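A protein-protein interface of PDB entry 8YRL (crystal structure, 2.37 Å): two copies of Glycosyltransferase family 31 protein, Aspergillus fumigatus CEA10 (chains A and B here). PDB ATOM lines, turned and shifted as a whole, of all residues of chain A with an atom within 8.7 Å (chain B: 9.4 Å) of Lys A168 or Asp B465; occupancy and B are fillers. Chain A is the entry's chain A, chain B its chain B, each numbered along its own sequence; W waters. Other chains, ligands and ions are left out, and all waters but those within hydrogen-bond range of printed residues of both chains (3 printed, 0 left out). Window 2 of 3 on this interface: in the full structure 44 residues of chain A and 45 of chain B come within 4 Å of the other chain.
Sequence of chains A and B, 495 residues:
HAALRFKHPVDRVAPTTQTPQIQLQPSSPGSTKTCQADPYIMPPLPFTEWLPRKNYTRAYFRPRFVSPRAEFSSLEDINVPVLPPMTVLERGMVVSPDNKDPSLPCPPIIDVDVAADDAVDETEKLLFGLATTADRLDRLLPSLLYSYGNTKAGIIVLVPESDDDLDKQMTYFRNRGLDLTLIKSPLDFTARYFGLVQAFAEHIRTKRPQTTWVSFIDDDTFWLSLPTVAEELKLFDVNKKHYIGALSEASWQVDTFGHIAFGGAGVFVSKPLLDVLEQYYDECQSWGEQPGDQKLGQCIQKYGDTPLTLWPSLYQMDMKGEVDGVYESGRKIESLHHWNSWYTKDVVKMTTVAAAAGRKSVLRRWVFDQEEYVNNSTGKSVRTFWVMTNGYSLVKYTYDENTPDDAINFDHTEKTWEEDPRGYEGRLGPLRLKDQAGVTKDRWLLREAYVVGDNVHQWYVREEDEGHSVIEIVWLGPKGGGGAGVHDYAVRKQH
Among the printed residues, Asp or Glu carboxylates within 4 Å of a Lys or Arg side-chain nitrogen of the other chain: Lys A168 with Asp B465 and Arg A176 with Glu B463.
No position is printed for both chains.
The guanidinium group (NH1) of Arg A176 lies within hydrogen-bond range of the backbone carbonyl oxygen (O) of Tyr A172 (3.2 Å). OD1 of Asp A165 sits at hydrogen-bond distance from N of Lys A168 (3.4 Å). N of Asn B55 is in hydrogen-bond range of O of His B468, at 2.7 Å. The guanidinium group (NH2) of Arg B462 lies within salt-bridge range of the side-chain carboxylate (OE2) of Glu B464, 3.0 Å away. The guanidinium group of Arg A174 lies within hydrogen-bond range of the side-chain hydroxyl of Thr A171, 3.2 Å away. The side-chain carboxylate of Glu B463 is in hydrogen-bond range of a ring nitrogen (ND1) of His B468 (2.8 Å).
The backbone carbonyl oxygen of Glu B466 is in hydrogen-bond range of the side-chain amide nitrogen of Asn A175, 2.9 Å away. The guanidinium group (NH1) of Arg A176 lies within hydrogen-bond range of the backbone carbonyl oxygen (O) of Glu B464, 3.1 Å away. The backbone carbonyl oxygen of Gly B467 is in hydrogen-bond range of the guanidinium group of Arg A176 (3.2 Å). NZ of Lys A168 lies within salt-bridge range of OD2 of Asp B465. NH2 of Arg A176 lies within salt-bridge range of OE1 of Glu B463 (2.5 Å).
Water W1 lies within hydrogen-bond range of N of His B468 and O of Asn A175. Water W2 bridges the backbone carbonyl oxygen (O) of Asp B465 and the backbone carbonyl oxygen (O) of Lys A168. Water W3 lies within hydrogen-bond range of NE of Arg A176 (2.8 Å), OE1 of Glu B463 (2.9 Å) and ND1 of His B468 (3.2 Å).
Of chain B, only Asp B465 comes within 4 Å of Lys A168. Of chain A, only Lys A168 (3.4 Å) and Tyr A172 (3.8 Å) come within 4 Å of Asp B465. Of the printed residues of chain B, Tyr A172 touches Glu B463, Glu B464 and Asp B465. Printed residues of chain B within 4 Å of Arg A176: Glu B463 (2.5 Å), Glu B464 (3.1 Å), Gly B467 (3.2 Å) and His B468 (3.7 Å). Of the printed residues of chain A, Glu B466 touches Thr A171 and Asn A175. Printed residues of chain A within 4 Å of Gly B467: Arg A176 (3.2 Å). Printed residues of chain A within 4 Å of Glu B464: Tyr A172 (3.8 Å) and Arg A176 (3.1 Å). The nearest printed residue of chain A that does not touch His B468 is Asn A175 (5.4 Å).
Among the printed residues, pairs that only touch across the chains: Arg A176 with His B468 (3.7 Å), Tyr A172 with Glu B464 (3.8 Å), Tyr A172 with Glu B463 (3.8 Å), Tyr A172 with Asp B465 (3.8 Å) and Thr A171 with Glu B466 (3.9 Å).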
ATOM      1  N   ALA A 134      -8.295 -19.635  -2.130  1.00  0.00           N
ATOM      2  CA  ALA A 134      -8.546 -20.806  -1.299  1.00  0.00           C
ATOM      3  C   ALA A 134      -7.253 -21.522  -0.936  1.00  0.00           C
ATOM      4  O   ALA A 134      -7.178 -22.169   0.116  1.00  0.00           O
ATOM      5  CB  ALA A 134      -9.501 -21.763  -2.013  1.00  0.00           C
ATOM      6  N   ASP A 163     -12.467 -22.240 -12.203  1.00  0.00           N
ATOM      7  CA  ASP A 163     -13.429 -23.330 -12.291  1.00  0.00           C
ATOM      8  C   ASP A 163     -13.647 -24.023 -10.952  1.00  0.00           C
ATOM      9  O   ASP A 163     -14.291 -25.077 -10.912  1.00  0.00           O
ATOM     10  CB  ASP A 163     -12.970 -24.356 -13.333  1.00  0.00           C
ATOM     11  CG  ASP A 163     -12.938 -23.790 -14.739  1.00  0.00           C
ATOM     12  OD1 ASP A 163     -13.837 -22.994 -15.084  1.00  0.00           O
ATOM     13  OD2 ASP A 163     -12.012 -24.142 -15.500  1.00  0.00           O
ATOM     14  N   ASP A 164     -13.125 -23.460  -9.866  1.00  0.00           N
ATOM     15  CA  ASP A 164     -13.196 -24.113  -8.567  1.00  0.00           C
ATOM     16  C   ASP A 164     -14.632 -24.182  -8.065  1.00  0.00           C
ATOM     17  O   ASP A 164     -15.400 -23.222  -8.188  1.00  0.00           O
ATOM     18  CB  ASP A 164     -12.329 -23.371  -7.549  1.00  0.00           C
ATOM     19  CG  ASP A 164     -10.859 -23.380  -7.917  1.00  0.00           C
ATOM     20  OD1 ASP A 164     -10.512 -23.953  -8.971  1.00  0.00           O
ATOM     21  OD2 ASP A 164     -10.052 -22.809  -7.154  1.00  0.00           O
ATOM     22  N   ASP A 165     -14.990 -25.328  -7.495  1.00  0.00           N
ATOM     23  CA  ASP A 165     -16.289 -25.495  -6.854  1.00  0.00           C
ATOM     24  C   ASP A 165     -16.279 -24.745  -5.528  1.00  0.00           C
ATOM     25  O   ASP A 165     -15.658 -25.192  -4.558  1.00  0.00           O
ATOM     26  CB  ASP A 165     -16.590 -26.976  -6.648  1.00  0.00           C
ATOM     27  CG  ASP A 165     -18.049 -27.241  -6.313  1.00  0.00           C
ATOM     28  OD1 ASP A 165     -18.760 -26.293  -5.916  1.00  0.00           O
ATOM     29  OD2 ASP A 165     -18.484 -28.404  -6.443  1.00  0.00           O
ATOM     30  N   LEU A 166     -16.962 -23.599  -5.483  1.00  0.00           N
ATOM     31  CA  LEU A 166     -16.976 -22.798  -4.263  1.00  0.00           C
ATOM     32  C   LEU A 166     -17.701 -23.522  -3.135  1.00  0.00           C
ATOM     33  O   LEU A 166     -17.297 -23.422  -1.970  1.00  0.00           O
ATOM     34  CB  LEU A 166     -17.621 -21.438  -4.532  1.00  0.00           C
ATOM     35  CG  LEU A 166     -16.902 -20.537  -5.537  1.00  0.00           C
ATOM     36  CD1 LEU A 166     -17.619 -19.202  -5.680  1.00  0.00           C
ATOM     37  CD2 LEU A 166     -15.450 -20.329  -5.134  1.00  0.00           C
ATOM     38  N   ASP A 167     -18.768 -24.257  -3.458  1.00  0.00           N
ATOM     39  CA  ASP A 167     -19.503 -24.982  -2.427  1.00  0.00           C
ATOM     40  C   ASP A 167     -18.657 -26.097  -1.826  1.00  0.00           C
ATOM     41  O   ASP A 167     -18.709 -26.337  -0.615  1.00  0.00           O
ATOM     42  CB  ASP A 167     -20.801 -25.544  -3.006  1.00  0.00           C
ATOM     43  CG  ASP A 167     -21.785 -24.457  -3.396  1.00  0.00           C
ATOM     44  OD1 ASP A 167     -21.905 -23.465  -2.646  1.00  0.00           O
ATOM     45  OD2 ASP A 167     -22.435 -24.592  -4.453  1.00  0.00           O
ATOM     46  N   LYS A 168     -17.872 -26.787  -2.656  1.00  0.00           N
ATOM     47  CA  LYS A 168     -16.996 -27.835  -2.144  1.00  0.00           C
ATOM     48  C   LYS A 168     -15.867 -27.249  -1.305  1.00  0.00           C
ATOM     49  O   LYS A 168     -15.546 -27.775  -0.233  1.00  0.00           O
ATOM     50  CB  LYS A 168     -16.437 -28.661  -3.302  1.00  0.00           C
ATOM     51  CG  LYS A 168     -15.178 -29.445  -2.967  1.00  0.00           C
ATOM     52  CD  LYS A 168     -15.093 -30.724  -3.783  1.00  0.00           C
ATOM     53  CE  LYS A 168     -14.041 -30.617  -4.877  1.00  0.00           C
ATOM     54  NZ  LYS A 168     -13.205 -31.847  -4.957  1.00  0.00           N
ATOM     55  N   GLN A 169     -15.254 -26.161  -1.777  1.00  0.00           N
ATOM     56  CA  GLN A 169     -14.191 -25.521  -1.010  1.00  0.00           C
ATOM     57  C   GLN A 169     -14.726 -24.948   0.296  1.00  0.00           C
ATOM     58  O   GLN A 169     -14.049 -24.999   1.330  1.00  0.00           O
ATOM     59  CB  GLN A 169     -13.529 -24.422  -1.842  1.00  0.00           C
ATOM     60  CG  GLN A 169     -12.603 -24.927  -2.937  1.00  0.00           C
ATOM     61  CD  GLN A 169     -12.071 -23.804  -3.807  1.00  0.00           C
ATOM     62  OE1 GLN A 169     -12.664 -22.727  -3.878  1.00  0.00           O
ATOM     63  NE2 GLN A 169     -10.948 -24.048  -4.472  1.00  0.00           N
ATOM     64  N   MET A 170     -15.940 -24.396   0.267  1.00  0.00           N
ATOM     65  CA  MET A 170     -16.534 -23.835   1.477  1.00  0.00           C
ATOM     66  C   MET A 170     -16.812 -24.923   2.506  1.00  0.00           C
ATOM     67  O   MET A 170     -16.626 -24.709   3.710  1.00  0.00           O
ATOM     68  CB  MET A 170     -17.817 -23.084   1.124  1.00  0.00           C
ATOM     69  CG  MET A 170     -17.666 -21.573   1.093  1.00  0.00           C
ATOM     70  SD  MET A 170     -19.251 -20.734   0.920  1.00  0.00           S
ATOM     71  CE  MET A 170     -19.549 -20.945  -0.832  1.00  0.00           C
ATOM     72  N   THR A 171     -17.258 -26.096   2.051  1.00  0.00           N
ATOM     73  CA  THR A 171     -17.471 -27.215   2.963  1.00  0.00           C
ATOM     74  C   THR A 171     -16.149 -27.715   3.534  1.00  0.00           C
ATOM     75  O   THR A 171     -16.078 -28.102   4.706  1.00  0.00           O
ATOM     76  CB  THR A 171     -18.209 -28.341   2.235  1.00  0.00           C
ATOM     77  OG1 THR A 171     -19.507 -27.882   1.836  1.00  0.00           O
ATOM     78  CG2 THR A 171     -18.366 -29.558   3.136  1.00  0.00           C
ATOM     79  N   TYR A 172     -15.090 -27.698   2.719  1.00  0.00           N
ATOM     80  CA  TYR A 172     -13.775 -28.129   3.182  1.00  0.00           C
ATOM     81  C   TYR A 172     -13.318 -27.315   4.387  1.00  0.00           C
ATOM     82  O   TYR A 172     -12.754 -27.865   5.341  1.00  0.00           O
ATOM     83  CB  TYR A 172     -12.766 -28.017   2.036  1.00  0.00           C
ATOM     84  CG  TYR A 172     -11.342 -28.388   2.394  1.00  0.00           C
ATOM     85  CD1 TYR A 172     -10.459 -27.441   2.901  1.00  0.00           C
ATOM     86  CD2 TYR A 172     -10.875 -29.682   2.206  1.00  0.00           C
ATOM     87  CE1 TYR A 172      -9.158 -27.776   3.223  1.00  0.00           C
ATOM     88  CE2 TYR A 172      -9.575 -30.025   2.522  1.00  0.00           C
ATOM     89  CZ  TYR A 172      -8.721 -29.070   3.031  1.00  0.00           C
ATOM     90  OH  TYR A 172      -7.426 -29.409   3.350  1.00  0.00           O
ATOM     91  N   PHE A 173     -13.558 -26.002   4.367  1.00  0.00           N
ATOM     92  CA  PHE A 173     -13.123 -25.148   5.465  1.00  0.00           C
ATOM     93  C   PHE A 173     -14.107 -25.177   6.629  1.00  0.00           C
ATOM     94  O   PHE A 173     -13.694 -25.141   7.794  1.00  0.00           O
ATOM     95  CB  PHE A 173     -12.930 -23.715   4.969  1.00  0.00           C
ATOM     96  CG  PHE A 173     -11.699 -23.523   4.132  1.00  0.00           C
ATOM     97  CD1 PHE A 173     -10.438 -23.675   4.686  1.00  0.00           C
ATOM     98  CD2 PHE A 173     -11.801 -23.194   2.791  1.00  0.00           C
ATOM     99  CE1 PHE A 173      -9.303 -23.500   3.917  1.00  0.00           C
ATOM    100  CE2 PHE A 173     -10.670 -23.019   2.016  1.00  0.00           C
ATOM    101  CZ  PHE A 173      -9.419 -23.173   2.581  1.00  0.00           C
ATOM    102  N   ARG A 174     -15.409 -25.239   6.334  1.00  0.00           N
ATOM    103  CA  ARG A 174     -16.412 -25.212   7.394  1.00  0.00           C
ATOM    104  C   ARG A 174     -16.331 -26.456   8.269  1.00  0.00           C
ATOM    105  O   ARG A 174     -16.427 -26.362   9.499  1.00  0.00           O
ATOM    106  CB  ARG A 174     -17.809 -25.072   6.790  1.00  0.00           C
ATOM    107  CG  ARG A 174     -18.938 -25.216   7.798  1.00  0.00           C
ATOM    108  CD  ARG A 174     -20.262 -25.496   7.106  1.00  0.00           C
ATOM    109  NE  ARG A 174     -20.331 -24.873   5.790  1.00  0.00           N
ATOM    110  CZ  ARG A 174     -20.521 -25.533   4.657  1.00  0.00           C
ATOM    111  NH1 ARG A 174     -20.667 -26.849   4.639  1.00  0.00           N
ATOM    112  NH2 ARG A 174     -20.566 -24.859   3.512  1.00  0.00           N
ATOM    113  N   ASN A 175     -16.159 -27.629   7.657  1.00  0.00           N
ATOM    114  CA  ASN A 175     -16.039 -28.859   8.432  1.00  0.00           C
ATOM    115  C   ASN A 175     -14.799 -28.863   9.314  1.00  0.00           C
ATOM    116  O   ASN A 175     -14.766 -29.585  10.315  1.00  0.00           O
ATOM    117  CB  ASN A 175     -16.025 -30.070   7.499  1.00  0.00           C
ATOM    118  CG  ASN A 175     -17.383 -30.348   6.884  1.00  0.00           C
ATOM    119  OD1 ASN A 175     -18.379 -29.721   7.246  1.00  0.00           O
ATOM    120  ND2 ASN A 175     -17.430 -31.291   5.951  1.00  0.00           N
ATOM    121  N   ARG A 176     -13.785 -28.070   8.971  1.00  0.00           N
ATOM    122  CA  ARG A 176     -12.582 -27.963   9.783  1.00  0.00           C
ATOM    123  C   ARG A 176     -12.685 -26.891  10.860  1.00  0.00           C
ATOM    124  O   ARG A 176     -11.804 -26.816  11.723  1.00  0.00           O
ATOM    125  CB  ARG A 176     -11.369 -27.684   8.889  1.00  0.00           C
ATOM    126  CG  ARG A 176     -10.873 -28.914   8.147  1.00  0.00           C
ATOM    127  CD  ARG A 176      -9.984 -28.552   6.969  1.00  0.00           C
ATOM    128  NE  ARG A 176      -9.286 -29.721   6.448  1.00  0.00           N
ATOM    129  CZ  ARG A 176      -9.854 -30.675   5.723  1.00  0.00           C
ATOM    130  NH1 ARG A 176     -11.134 -30.619   5.387  1.00  0.00           N
ATOM    131  NH2 ARG A 176      -9.120 -31.705   5.315  1.00  0.00           N
ATOM    132  N   LEU A 182     -17.202 -17.913   0.062  1.00  0.00           N
ATOM    133  CA  LEU A 182     -16.301 -17.677  -1.058  1.00  0.00           C
ATOM    134  C   LEU A 182     -17.081 -17.086  -2.223  1.00  0.00           C
ATOM    135  O   LEU A 182     -18.103 -17.642  -2.639  1.00  0.00           O
ATOM    136  CB  LEU A 182     -15.609 -18.973  -1.483  1.00  0.00           C
ATOM    137  CG  LEU A 182     -14.684 -19.602  -0.441  1.00  0.00           C
ATOM    138  CD1 LEU A 182     -14.012 -20.849  -0.993  1.00  0.00           C
ATOM    139  CD2 LEU A 182     -13.648 -18.591   0.015  1.00  0.00           C
ATOM    140  N   ASN B  55     -12.086 -35.705  12.385  1.00  0.00           N
ATOM    141  CA  ASN B  55     -12.553 -37.068  12.578  1.00  0.00           C
ATOM    142  C   ASN B  55     -11.388 -37.896  13.111  1.00  0.00           C
ATOM    143  O   ASN B  55     -10.328 -37.959  12.478  1.00  0.00           O
ATOM    144  CB  ASN B  55     -13.087 -37.638  11.266  1.00  0.00           C
ATOM    145  CG  ASN B  55     -14.215 -36.805  10.687  1.00  0.00           C
ATOM    146  OD1 ASN B  55     -15.220 -36.553  11.354  1.00  0.00           O
ATOM    147  ND2 ASN B  55     -14.054 -36.370   9.443  1.00  0.00           N
ATOM    148  N   ARG B 462      -5.194 -37.631   6.977  1.00  0.00           N
ATOM    149  CA  ARG B 462      -5.679 -37.542   5.605  1.00  0.00           C
ATOM    150  C   ARG B 462      -6.629 -36.358   5.506  1.00  0.00           C
ATOM    151  O   ARG B 462      -7.589 -36.262   6.276  1.00  0.00           O
ATOM    152  CB  ARG B 462      -6.391 -38.824   5.166  1.00  0.00           C
ATOM    153  CG  ARG B 462      -6.957 -38.736   3.754  1.00  0.00           C
ATOM    154  CD  ARG B 462      -7.266 -40.104   3.173  1.00  0.00           C
ATOM    155  NE  ARG B 462      -8.699 -40.369   3.136  1.00  0.00           N
ATOM    156  CZ  ARG B 462      -9.434 -40.346   2.032  1.00  0.00           C
ATOM    157  NH1 ARG B 462      -8.905 -40.063   0.852  1.00  0.00           N
ATOM    158  NH2 ARG B 462     -10.735 -40.614   2.114  1.00  0.00           N
ATOM    159  N   GLU B 463      -6.359 -35.460   4.560  1.00  0.00           N
ATOM    160  CA  GLU B 463      -7.175 -34.260   4.379  1.00  0.00           C
ATOM    161  C   GLU B 463      -8.298 -34.585   3.402  1.00  0.00           C
ATOM    162  O   GLU B 463      -8.179 -34.386   2.194  1.00  0.00           O
ATOM    163  CB  GLU B 463      -6.322 -33.096   3.891  1.00  0.00           C
ATOM    164  CG  GLU B 463      -5.164 -32.733   4.813  1.00  0.00           C
ATOM    165  CD  GLU B 463      -5.589 -31.900   6.009  1.00  0.00           C
ATOM    166  OE1 GLU B 463      -6.808 -31.753   6.244  1.00  0.00           O
ATOM    167  OE2 GLU B 463      -4.699 -31.386   6.717  1.00  0.00           O
ATOM    168  N   GLU B 464      -9.407 -35.088   3.937  1.00  0.00           N
ATOM    169  CA  GLU B 464     -10.555 -35.418   3.110  1.00  0.00           C
ATOM    170  C   GLU B 464     -11.406 -34.178   2.852  1.00  0.00           C
ATOM    171  O   GLU B 464     -11.326 -33.174   3.566  1.00  0.00           O
ATOM    172  CB  GLU B 464     -11.405 -36.505   3.771  1.00  0.00           C
ATOM    173  CG  GLU B 464     -10.609 -37.707   4.249  1.00  0.00           C
ATOM    174  CD  GLU B 464     -11.460 -38.701   5.012  1.00  0.00           C
ATOM    175  OE1 GLU B 464     -12.426 -38.274   5.680  1.00  0.00           O
ATOM    176  OE2 GLU B 464     -11.161 -39.912   4.948  1.00  0.00           O
ATOM    177  N   ASP B 465     -12.232 -34.261   1.806  1.00  0.00           N
ATOM    178  CA  ASP B 465     -13.124 -33.158   1.466  1.00  0.00           C
ATOM    179  C   ASP B 465     -14.150 -32.895   2.558  1.00  0.00           C
ATOM    180  O   ASP B 465     -14.651 -31.770   2.663  1.00  0.00           O
ATOM    181  CB  ASP B 465     -13.835 -33.445   0.142  1.00  0.00           C
ATOM    182  CG  ASP B 465     -12.900 -33.373  -1.052  1.00  0.00           C
ATOM    183  OD1 ASP B 465     -11.733 -32.969  -0.873  1.00  0.00           O
ATOM    184  OD2 ASP B 465     -13.335 -33.717  -2.170  1.00  0.00           O
ATOM    185  N   GLU B 466     -14.470 -33.899   3.373  1.00  0.00           N
ATOM    186  CA  GLU B 466     -15.467 -33.765   4.423  1.00  0.00           C
ATOM    187  C   GLU B 466     -14.865 -33.442   5.783  1.00  0.00           C
ATOM    188  O   GLU B 466     -15.604 -33.387   6.771  1.00  0.00           O
ATOM    189  CB  GLU B 466     -16.305 -35.043   4.521  1.00  0.00           C
ATOM    190  CG  GLU B 466     -17.304 -35.221   3.390  1.00  0.00           C
ATOM    191  CD  GLU B 466     -18.413 -34.188   3.422  1.00  0.00           C
ATOM    192  OE1 GLU B 466     -19.201 -34.183   4.392  1.00  0.00           O
ATOM    193  OE2 GLU B 466     -18.496 -33.376   2.476  1.00  0.00           O
ATOM    194  N   GLY B 467     -13.561 -33.239   5.868  1.00  0.00           N
ATOM    195  CA  GLY B 467     -12.964 -32.787   7.109  1.00  0.00           C
ATOM    196  C   GLY B 467     -11.563 -33.336   7.292  1.00  0.00           C
ATOM    197  O   GLY B 467     -11.032 -34.065   6.459  1.00  0.00           O
ATOM    198  N   HIS B 468     -10.975 -32.951   8.422  1.00  0.00           N
ATOM    199  CA  HIS B 468      -9.643 -33.389   8.819  1.00  0.00           C
ATOM    200  C   HIS B 468      -9.738 -34.781   9.436  1.00  0.00           C
ATOM    201  O   HIS B 468     -10.374 -34.958  10.478  1.00  0.00           O
ATOM    202  CB  HIS B 468      -9.057 -32.384   9.812  1.00  0.00           C
ATOM    203  CG  HIS B 468      -7.579 -32.500  10.011  1.00  0.00           C
ATOM    204  ND1 HIS B 468      -6.663 -32.082   9.067  1.00  0.00           N
ATOM    205  CD2 HIS B 468      -6.853 -32.956  11.060  1.00  0.00           C
ATOM    206  CE1 HIS B 468      -5.440 -32.292   9.520  1.00  0.00           C
ATOM    207  NE2 HIS B 468      -5.528 -32.821  10.727  1.00  0.00           N
ATOM    208  N   SER B 469      -9.120 -35.769   8.794  1.00  0.00           N
ATOM    209  CA  SER B 469      -9.203 -37.159   9.232  1.00  0.00           C
ATOM    210  C   SER B 469      -7.901 -37.549   9.919  1.00  0.00           C
ATOM    211  O   SER B 469      -6.825 -37.456   9.318  1.00  0.00           O
ATOM    212  CB  SER B 469      -9.490 -38.088   8.052  1.00  0.00           C
ATOM    213  OG  SER B 469      -9.360 -39.447   8.429  1.00  0.00           O
HETATM  214  O   HOH W   1     -12.339 -31.452  10.135  1.00  0.00           O
HETATM  215  O   HOH W   2     -15.228 -30.503   0.320  1.00  0.00           O
HETATM  216  O   HOH W   3      -6.752 -29.271   7.647  1.00  0.00           O
